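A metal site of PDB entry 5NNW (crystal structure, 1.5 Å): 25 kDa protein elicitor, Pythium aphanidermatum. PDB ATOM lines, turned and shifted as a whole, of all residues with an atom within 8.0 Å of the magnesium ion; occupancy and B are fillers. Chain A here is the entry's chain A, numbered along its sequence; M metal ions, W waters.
Four residues have an atom within 4 Å of the magnesium ion: Asp 93, Asp 104, Glu 106 and His 159.
Water W1 binds the magnesium ion. The magnesium ion is bound by OE2 of Glu 106. The magnesium ion is bound by O of His 159, 2.1 Å away. The side-chain carboxylate (OD2) of Asp 93 binds the magnesium ion (2.2 Å). The side-chain carboxylate (OD2) of Asp 104 binds the magnesium ion, 2.3 Å away. The magnesium ion is bound by OD1 of Asp 104 (2.3 Å).
N of Asp 93 lies within hydrogen-bond range of O of His 101 (2.9 Å). The backbone NH (N) of Asp 104 lies within hydrogen-bond range of the backbone carbonyl oxygen (O) of Met 90 (2.9 Å). OD2 of Asp 104 sits close to OH of Tyr 151 (2.7 Å). N of Trp 88 lies within hydrogen-bond range of O of Glu 106 (3.0 Å). The side-chain carboxylate (OE1) of Glu 106 is in hydrogen-bond range of the side-chain hydroxyl (OG) of Ser 126 (2.8 Å).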
ATOM      1  N   TRP A  88     -23.487 -11.820  -4.955  1.00  0.00           N
ATOM      2  CA  TRP A  88     -23.007 -10.461  -4.689  1.00  0.00           C
ATOM      3  C   TRP A  88     -21.486 -10.428  -4.730  1.00  0.00           C
ATOM      4  O   TRP A  88     -20.815 -11.392  -4.313  1.00  0.00           O
ATOM      5  CB  TRP A  88     -23.485  -9.941  -3.318  1.00  0.00           C
ATOM      6  CG  TRP A  88     -24.963  -9.833  -3.174  1.00  0.00           C
ATOM      7  CD1 TRP A  88     -25.738  -8.742  -3.462  1.00  0.00           C
ATOM      8  CD2 TRP A  88     -25.853 -10.836  -2.671  1.00  0.00           C
ATOM      9  NE1 TRP A  88     -27.055  -9.010  -3.181  1.00  0.00           N
ATOM     10  CE2 TRP A  88     -27.161 -10.294  -2.701  1.00  0.00           C
ATOM     11  CE3 TRP A  88     -25.685 -12.148  -2.225  1.00  0.00           C
ATOM     12  CZ2 TRP A  88     -28.295 -11.011  -2.288  1.00  0.00           C
ATOM     13  CZ3 TRP A  88     -26.805 -12.874  -1.816  1.00  0.00           C
ATOM     14  CH2 TRP A  88     -28.092 -12.292  -1.840  1.00  0.00           C
ATOM     15  N   MET A  90     -18.270  -8.060  -3.405  1.00  0.00           N
ATOM     16  CA  MET A  90     -17.805  -6.981  -2.555  1.00  0.00           C
ATOM     17  C   MET A  90     -16.350  -6.667  -2.887  1.00  0.00           C
ATOM     18  O   MET A  90     -15.593  -7.565  -3.260  1.00  0.00           O
ATOM     19  CB  MET A  90     -17.935  -7.336  -1.069  1.00  0.00           C
ATOM     20  CG  MET A  90     -19.315  -7.155  -0.496  1.00  0.00           C
ATOM     21  SD  MET A  90     -20.540  -8.314  -1.157  1.00  0.00           S
ATOM     22  CE  MET A  90     -21.906  -8.049  -0.032  1.00  0.00           C
ATOM     23  N   LYS A  92     -13.742  -6.089  -1.120  1.00  0.00           N
ATOM     24  CA  LYS A  92     -12.774  -6.807  -0.297  1.00  0.00           C
ATOM     25  C   LYS A  92     -13.553  -7.619   0.717  1.00  0.00           C
ATOM     26  O   LYS A  92     -14.750  -7.412   0.919  1.00  0.00           O
ATOM     27  CB  LYS A  92     -11.795  -5.862   0.413  1.00  0.00           C
ATOM     28  CG  LYS A  92     -12.476  -4.855   1.320  1.00  0.00           C
ATOM     29  CD  LYS A  92     -11.443  -4.037   2.107  1.00  0.00           C
ATOM     30  CE  LYS A  92     -12.136  -2.959   2.913  1.00  0.00           C
ATOM     31  NZ  LYS A  92     -11.211  -2.217   3.799  1.00  0.00           N
ATOM     32  N   ASP A  93     -12.832  -8.542   1.365  1.00  0.00           N
ATOM     33  CA  ASP A  93     -13.351  -9.376   2.446  1.00  0.00           C
ATOM     34  C   ASP A  93     -12.270  -9.295   3.523  1.00  0.00           C
ATOM     35  O   ASP A  93     -11.328 -10.094   3.501  1.00  0.00           O
ATOM     36  CB  ASP A  93     -13.602 -10.809   1.988  1.00  0.00           C
ATOM     37  CG  ASP A  93     -14.301 -11.657   3.036  1.00  0.00           C
ATOM     38  OD1 ASP A  93     -14.330 -11.253   4.224  1.00  0.00           O
ATOM     39  OD2 ASP A  93     -14.840 -12.727   2.685  1.00  0.00           O
ATOM     40  N   SER A  94     -12.392  -8.332   4.418  1.00  0.00           N
ATOM     41  CA  SER A  94     -11.330  -8.043   5.392  1.00  0.00           C
ATOM     42  C   SER A  94     -11.929  -7.926   6.794  1.00  0.00           C
ATOM     43  O   SER A  94     -12.465  -6.871   7.159  1.00  0.00           O
ATOM     44  CB  SER A  94     -10.594  -6.769   5.006  1.00  0.00           C
ATOM     45  OG  SER A  94      -9.504  -6.528   5.877  1.00  0.00           O
ATOM     46  N   HIS A 101      -8.730 -10.392   2.252  1.00  0.00           N
ATOM     47  CA  HIS A 101      -8.189 -10.319   0.917  1.00  0.00           C
ATOM     48  C   HIS A 101      -9.030  -9.398   0.056  1.00  0.00           C
ATOM     49  O   HIS A 101     -10.176  -9.066   0.377  1.00  0.00           O
ATOM     50  CB  HIS A 101      -8.112 -11.700   0.262  1.00  0.00           C
ATOM     51  CG  HIS A 101      -9.390 -12.469   0.309  1.00  0.00           C
ATOM     52  ND1 HIS A 101     -10.459 -12.183  -0.518  1.00  0.00           N
ATOM     53  CD2 HIS A 101      -9.768 -13.527   1.063  1.00  0.00           C
ATOM     54  CE1 HIS A 101     -11.449 -13.025  -0.267  1.00  0.00           C
ATOM     55  NE2 HIS A 101     -11.054 -13.855   0.701  1.00  0.00           N
ATOM     56  N   HIS A 103     -11.295  -8.598  -3.070  1.00  0.00           N
ATOM     57  CA  HIS A 103     -12.444  -9.257  -3.701  1.00  0.00           C
ATOM     58  C   HIS A 103     -13.227 -10.162  -2.751  1.00  0.00           C
ATOM     59  O   HIS A 103     -12.672 -10.782  -1.844  1.00  0.00           O
ATOM     60  CB  HIS A 103     -12.038 -10.097  -4.922  1.00  0.00           C
ATOM     61  CG  HIS A 103     -11.246  -9.347  -5.945  1.00  0.00           C
ATOM     62  ND1 HIS A 103     -11.724  -8.223  -6.578  1.00  0.00           N
ATOM     63  CD2 HIS A 103     -10.010  -9.564  -6.439  1.00  0.00           C
ATOM     64  CE1 HIS A 103     -10.817  -7.785  -7.429  1.00  0.00           C
ATOM     65  NE2 HIS A 103      -9.763  -8.580  -7.357  1.00  0.00           N
ATOM     66  N   ASP A 104     -14.533 -10.265  -2.999  1.00  0.00           N
ATOM     67  CA  ASP A 104     -15.389 -11.222  -2.307  1.00  0.00           C
ATOM     68  C   ASP A 104     -16.528 -11.585  -3.250  1.00  0.00           C
ATOM     69  O   ASP A 104     -17.114 -10.702  -3.884  1.00  0.00           O
ATOM     70  CB  ASP A 104     -15.962 -10.670  -0.986  1.00  0.00           C
ATOM     71  CG  ASP A 104     -16.376 -11.776  -0.013  1.00  0.00           C
ATOM     72  OD1 ASP A 104     -16.025 -12.951  -0.268  1.00  0.00           O
ATOM     73  OD2 ASP A 104     -17.048 -11.480   0.999  1.00  0.00           O
ATOM     74  N   TRP A 105     -16.819 -12.875  -3.343  1.00  0.00           N
ATOM     75  CA  TRP A 105     -17.954 -13.380  -4.106  1.00  0.00           C
ATOM     76  C   TRP A 105     -18.747 -14.300  -3.200  1.00  0.00           C
ATOM     77  O   TRP A 105     -18.196 -15.270  -2.672  1.00  0.00           O
ATOM     78  CB  TRP A 105     -17.499 -14.146  -5.356  1.00  0.00           C
ATOM     79  CG  TRP A 105     -17.171 -13.319  -6.549  1.00  0.00           C
ATOM     80  CD1 TRP A 105     -15.932 -13.050  -7.059  1.00  0.00           C
ATOM     81  CD2 TRP A 105     -18.113 -12.671  -7.415  1.00  0.00           C
ATOM     82  NE1 TRP A 105     -16.047 -12.255  -8.185  1.00  0.00           N
ATOM     83  CE2 TRP A 105     -17.371 -12.017  -8.432  1.00  0.00           C
ATOM     84  CE3 TRP A 105     -19.524 -12.595  -7.446  1.00  0.00           C
ATOM     85  CZ2 TRP A 105     -17.983 -11.289  -9.455  1.00  0.00           C
ATOM     86  CZ3 TRP A 105     -20.121 -11.858  -8.466  1.00  0.00           C
ATOM     87  CH2 TRP A 105     -19.350 -11.233  -9.465  1.00  0.00           C
ATOM     88  N   GLU A 106     -20.037 -14.019  -3.018  1.00  0.00           N
ATOM     89  CA  GLU A 106     -20.913 -14.850  -2.202  1.00  0.00           C
ATOM     90  C   GLU A 106     -22.163 -15.155  -3.004  1.00  0.00           C
ATOM     91  O   GLU A 106     -22.506 -14.428  -3.930  1.00  0.00           O
ATOM     92  CB  GLU A 106     -21.316 -14.158  -0.900  1.00  0.00           C
ATOM     93  CG  GLU A 106     -20.141 -13.671  -0.063  1.00  0.00           C
ATOM     94  CD  GLU A 106     -19.371 -14.800   0.589  1.00  0.00           C
ATOM     95  OE1 GLU A 106     -19.902 -15.932   0.720  1.00  0.00           O
ATOM     96  OE2 GLU A 106     -18.205 -14.563   0.977  1.00  0.00           O
ATOM     97  N   SER A 126     -23.872 -19.358   0.845  1.00  0.00           N
ATOM     98  CA  SER A 126     -22.443 -19.657   0.845  1.00  0.00           C
ATOM     99  C   SER A 126     -21.764 -19.254   2.148  1.00  0.00           C
ATOM    100  O   SER A 126     -22.006 -18.167   2.689  1.00  0.00           O
ATOM    101  CB  SER A 126     -21.747 -18.951  -0.340  1.00  0.00           C
ATOM    102  OG  SER A 126     -21.948 -17.545  -0.318  1.00  0.00           O
ATOM    103  N   ALA A 127     -20.889 -20.137   2.644  1.00  0.00           N
ATOM    104  CA  ALA A 127     -20.110 -19.872   3.852  1.00  0.00           C
ATOM    105  C   ALA A 127     -18.768 -20.591   3.754  1.00  0.00           C
ATOM    106  O   ALA A 127     -18.486 -21.306   2.782  1.00  0.00           O
ATOM    107  CB  ALA A 127     -20.892 -20.270   5.104  1.00  0.00           C
ATOM    108  N   HIS A 128     -17.930 -20.399   4.780  1.00  0.00           N
ATOM    109  CA  HIS A 128     -16.537 -20.828   4.673  1.00  0.00           C
ATOM    110  C   HIS A 128     -16.409 -22.342   4.630  1.00  0.00           C
ATOM    111  O   HIS A 128     -15.535 -22.880   3.939  1.00  0.00           O
ATOM    112  CB  HIS A 128     -15.710 -20.245   5.823  1.00  0.00           C
ATOM    113  CG  HIS A 128     -16.055 -20.801   7.179  1.00  0.00           C
ATOM    114  ND1 HIS A 128     -17.170 -20.397   7.879  1.00  0.00           N
ATOM    115  CD2 HIS A 128     -15.416 -21.700   7.969  1.00  0.00           C
ATOM    116  CE1 HIS A 128     -17.216 -21.038   9.034  1.00  0.00           C
ATOM    117  NE2 HIS A 128     -16.161 -21.832   9.106  1.00  0.00           N
ATOM    118  N   TYR A 151     -25.166 -10.723   5.372  1.00  0.00           N
ATOM    119  CA  TYR A 151     -23.748 -10.717   5.040  1.00  0.00           C
ATOM    120  C   TYR A 151     -22.996 -10.207   6.250  1.00  0.00           C
ATOM    121  O   TYR A 151     -23.257  -9.090   6.712  1.00  0.00           O
ATOM    122  CB  TYR A 151     -23.485  -9.844   3.815  1.00  0.00           C
ATOM    123  CG  TYR A 151     -22.046  -9.724   3.373  1.00  0.00           C
ATOM    124  CD1 TYR A 151     -21.428 -10.699   2.587  1.00  0.00           C
ATOM    125  CD2 TYR A 151     -21.294  -8.589   3.706  1.00  0.00           C
ATOM    126  CE1 TYR A 151     -20.115 -10.550   2.164  1.00  0.00           C
ATOM    127  CE2 TYR A 151     -19.995  -8.440   3.283  1.00  0.00           C
ATOM    128  CZ  TYR A 151     -19.398  -9.418   2.505  1.00  0.00           C
ATOM    129  OH  TYR A 151     -18.092  -9.285   2.069  1.00  0.00           O
ATOM    130  N   LYS A 152     -22.076 -11.015   6.771  1.00  0.00           N
ATOM    131  CA  LYS A 152     -21.518 -10.717   8.081  1.00  0.00           C
ATOM    132  C   LYS A 152     -20.221 -11.480   8.278  1.00  0.00           C
ATOM    133  O   LYS A 152     -20.093 -12.642   7.860  1.00  0.00           O
ATOM    134  CB  LYS A 152     -22.521 -11.097   9.186  1.00  0.00           C
ATOM    135  CG  LYS A 152     -22.006 -10.968  10.609  1.00  0.00           C
ATOM    136  CD  LYS A 152     -23.003 -11.525  11.617  1.00  0.00           C
ATOM    137  CE  LYS A 152     -22.413 -11.549  13.016  1.00  0.00           C
ATOM    138  NZ  LYS A 152     -23.393 -12.008  14.045  1.00  0.00           N
ATOM    139  N   SER A 153     -19.249 -10.826   8.910  1.00  0.00           N
ATOM    140  CA  SER A 153     -18.060 -11.490   9.423  1.00  0.00           C
ATOM    141  C   SER A 153     -18.201 -11.661  10.932  1.00  0.00           C
ATOM    142  O   SER A 153     -18.490 -10.689  11.644  1.00  0.00           O
ATOM    143  CB  SER A 153     -16.783 -10.703   9.125  1.00  0.00           C
ATOM    144  OG  SER A 153     -15.688 -11.154   9.935  1.00  0.00           O
ATOM    145  N   LEU A 157     -13.265 -14.773  11.125  1.00  0.00           N
ATOM    146  CA  LEU A 157     -13.624 -15.431   9.880  1.00  0.00           C
ATOM    147  C   LEU A 157     -14.023 -14.417   8.816  1.00  0.00           C
ATOM    148  O   LEU A 157     -14.436 -13.296   9.107  1.00  0.00           O
ATOM    149  CB  LEU A 157     -14.777 -16.407  10.130  1.00  0.00           C
ATOM    150  CG  LEU A 157     -14.442 -17.704  10.866  1.00  0.00           C
ATOM    151  CD1 LEU A 157     -15.695 -18.556  10.994  1.00  0.00           C
ATOM    152  CD2 LEU A 157     -13.337 -18.482  10.170  1.00  0.00           C
ATOM    153  N   ASP A 158     -13.899 -14.839   7.556  1.00  0.00           N
ATOM    154  CA  ASP A 158     -14.261 -13.983   6.430  1.00  0.00           C
ATOM    155  C   ASP A 158     -15.751 -13.654   6.468  1.00  0.00           C
ATOM    156  O   ASP A 158     -16.555 -14.364   7.067  1.00  0.00           O
ATOM    157  CB  ASP A 158     -13.938 -14.686   5.105  1.00  0.00           C
ATOM    158  CG  ASP A 158     -12.443 -14.702   4.768  1.00  0.00           C
ATOM    159  OD1 ASP A 158     -11.646 -14.129   5.546  1.00  0.00           O
ATOM    160  OD2 ASP A 158     -12.079 -15.266   3.728  1.00  0.00           O
ATOM    161  N   HIS A 159     -16.110 -12.547   5.813  1.00  0.00           N
ATOM    162  CA  HIS A 159     -17.522 -12.203   5.633  1.00  0.00           C
ATOM    163  C   HIS A 159     -18.193 -13.244   4.756  1.00  0.00           C
ATOM    164  O   HIS A 159     -17.704 -13.568   3.661  1.00  0.00           O
ATOM    165  CB  HIS A 159     -17.680 -10.829   4.991  1.00  0.00           C
ATOM    166  CG  HIS A 159     -17.092  -9.698   5.777  1.00  0.00           C
ATOM    167  ND1 HIS A 159     -15.743  -9.421   5.785  1.00  0.00           N
ATOM    168  CD2 HIS A 159     -17.673  -8.758   6.570  1.00  0.00           C
ATOM    169  CE1 HIS A 159     -15.510  -8.372   6.562  1.00  0.00           C
ATOM    170  NE2 HIS A 159     -16.667  -7.951   7.045  1.00  0.00           N
ATOM    171  N   GLU A 160     -19.344 -13.742   5.214  1.00  0.00           N
ATOM    172  CA  GLU A 160     -20.053 -14.812   4.532  1.00  0.00           C
ATOM    173  C   GLU A 160     -21.558 -14.600   4.686  1.00  0.00           C
ATOM    174  O   GLU A 160     -22.017 -13.712   5.407  1.00  0.00           O
ATOM    175  CB  GLU A 160     -19.652 -16.175   5.096  1.00  0.00           C
ATOM    176  CG  GLU A 160     -20.123 -16.343   6.536  1.00  0.00           C
ATOM    177  CD  GLU A 160     -19.691 -17.669   7.142  1.00  0.00           C
ATOM    178  OE1 GLU A 160     -18.620 -18.178   6.760  1.00  0.00           O
ATOM    179  OE2 GLU A 160     -20.448 -18.181   8.009  1.00  0.00           O
ATOM    180  N   LEU A 161     -22.344 -15.432   4.000  1.00  0.00           N
ATOM    181  CA  LEU A 161     -23.786 -15.284   4.036  1.00  0.00           C
ATOM    182  C   LEU A 161     -24.412 -16.147   5.119  1.00  0.00           C
ATOM    183  O   LEU A 161     -23.814 -17.105   5.611  1.00  0.00           O
ATOM    184  CB  LEU A 161     -24.398 -15.635   2.672  1.00  0.00           C
ATOM    185  CG  LEU A 161     -23.928 -14.813   1.484  1.00  0.00           C
ATOM    186  CD1 LEU A 161     -24.647 -15.255   0.229  1.00  0.00           C
ATOM    187  CD2 LEU A 161     -24.136 -13.328   1.725  1.00  0.00           C
ATOM    188  N   ASN A 194      -8.383 -14.787  -4.197  1.00  0.00           N
ATOM    189  CA  ASN A 194      -8.965 -15.670  -3.207  1.00  0.00           C
ATOM    190  C   ASN A 194     -10.465 -15.839  -3.377  1.00  0.00           C
ATOM    191  O   ASN A 194     -11.037 -16.765  -2.788  1.00  0.00           O
ATOM    192  CB  ASN A 194      -8.648 -15.128  -1.815  1.00  0.00           C
ATOM    193  CG  ASN A 194      -7.155 -15.159  -1.508  1.00  0.00           C
ATOM    194  OD1 ASN A 194      -6.565 -16.230  -1.345  1.00  0.00           O
ATOM    195  ND2 ASN A 194      -6.535 -13.991  -1.457  1.00  0.00           N
ATOM    196  N   ALA A 195     -11.117 -14.978  -4.150  1.00  0.00           N
ATOM    197  CA  ALA A 195     -12.543 -15.064  -4.407  1.00  0.00           C
ATOM    198  C   ALA A 195     -12.780 -15.745  -5.743  1.00  0.00           C
ATOM    199  O   ALA A 195     -11.914 -15.734  -6.622  1.00  0.00           O
ATOM    200  CB  ALA A 195     -13.178 -13.670  -4.402  1.00  0.00           C
HETATM  201 MG    MG M   1     -16.647 -13.574   1.865  1.00  0.00          MG
HETATM  202  O   HOH W   1     -15.510 -15.215   1.768  1.00  0.00           O
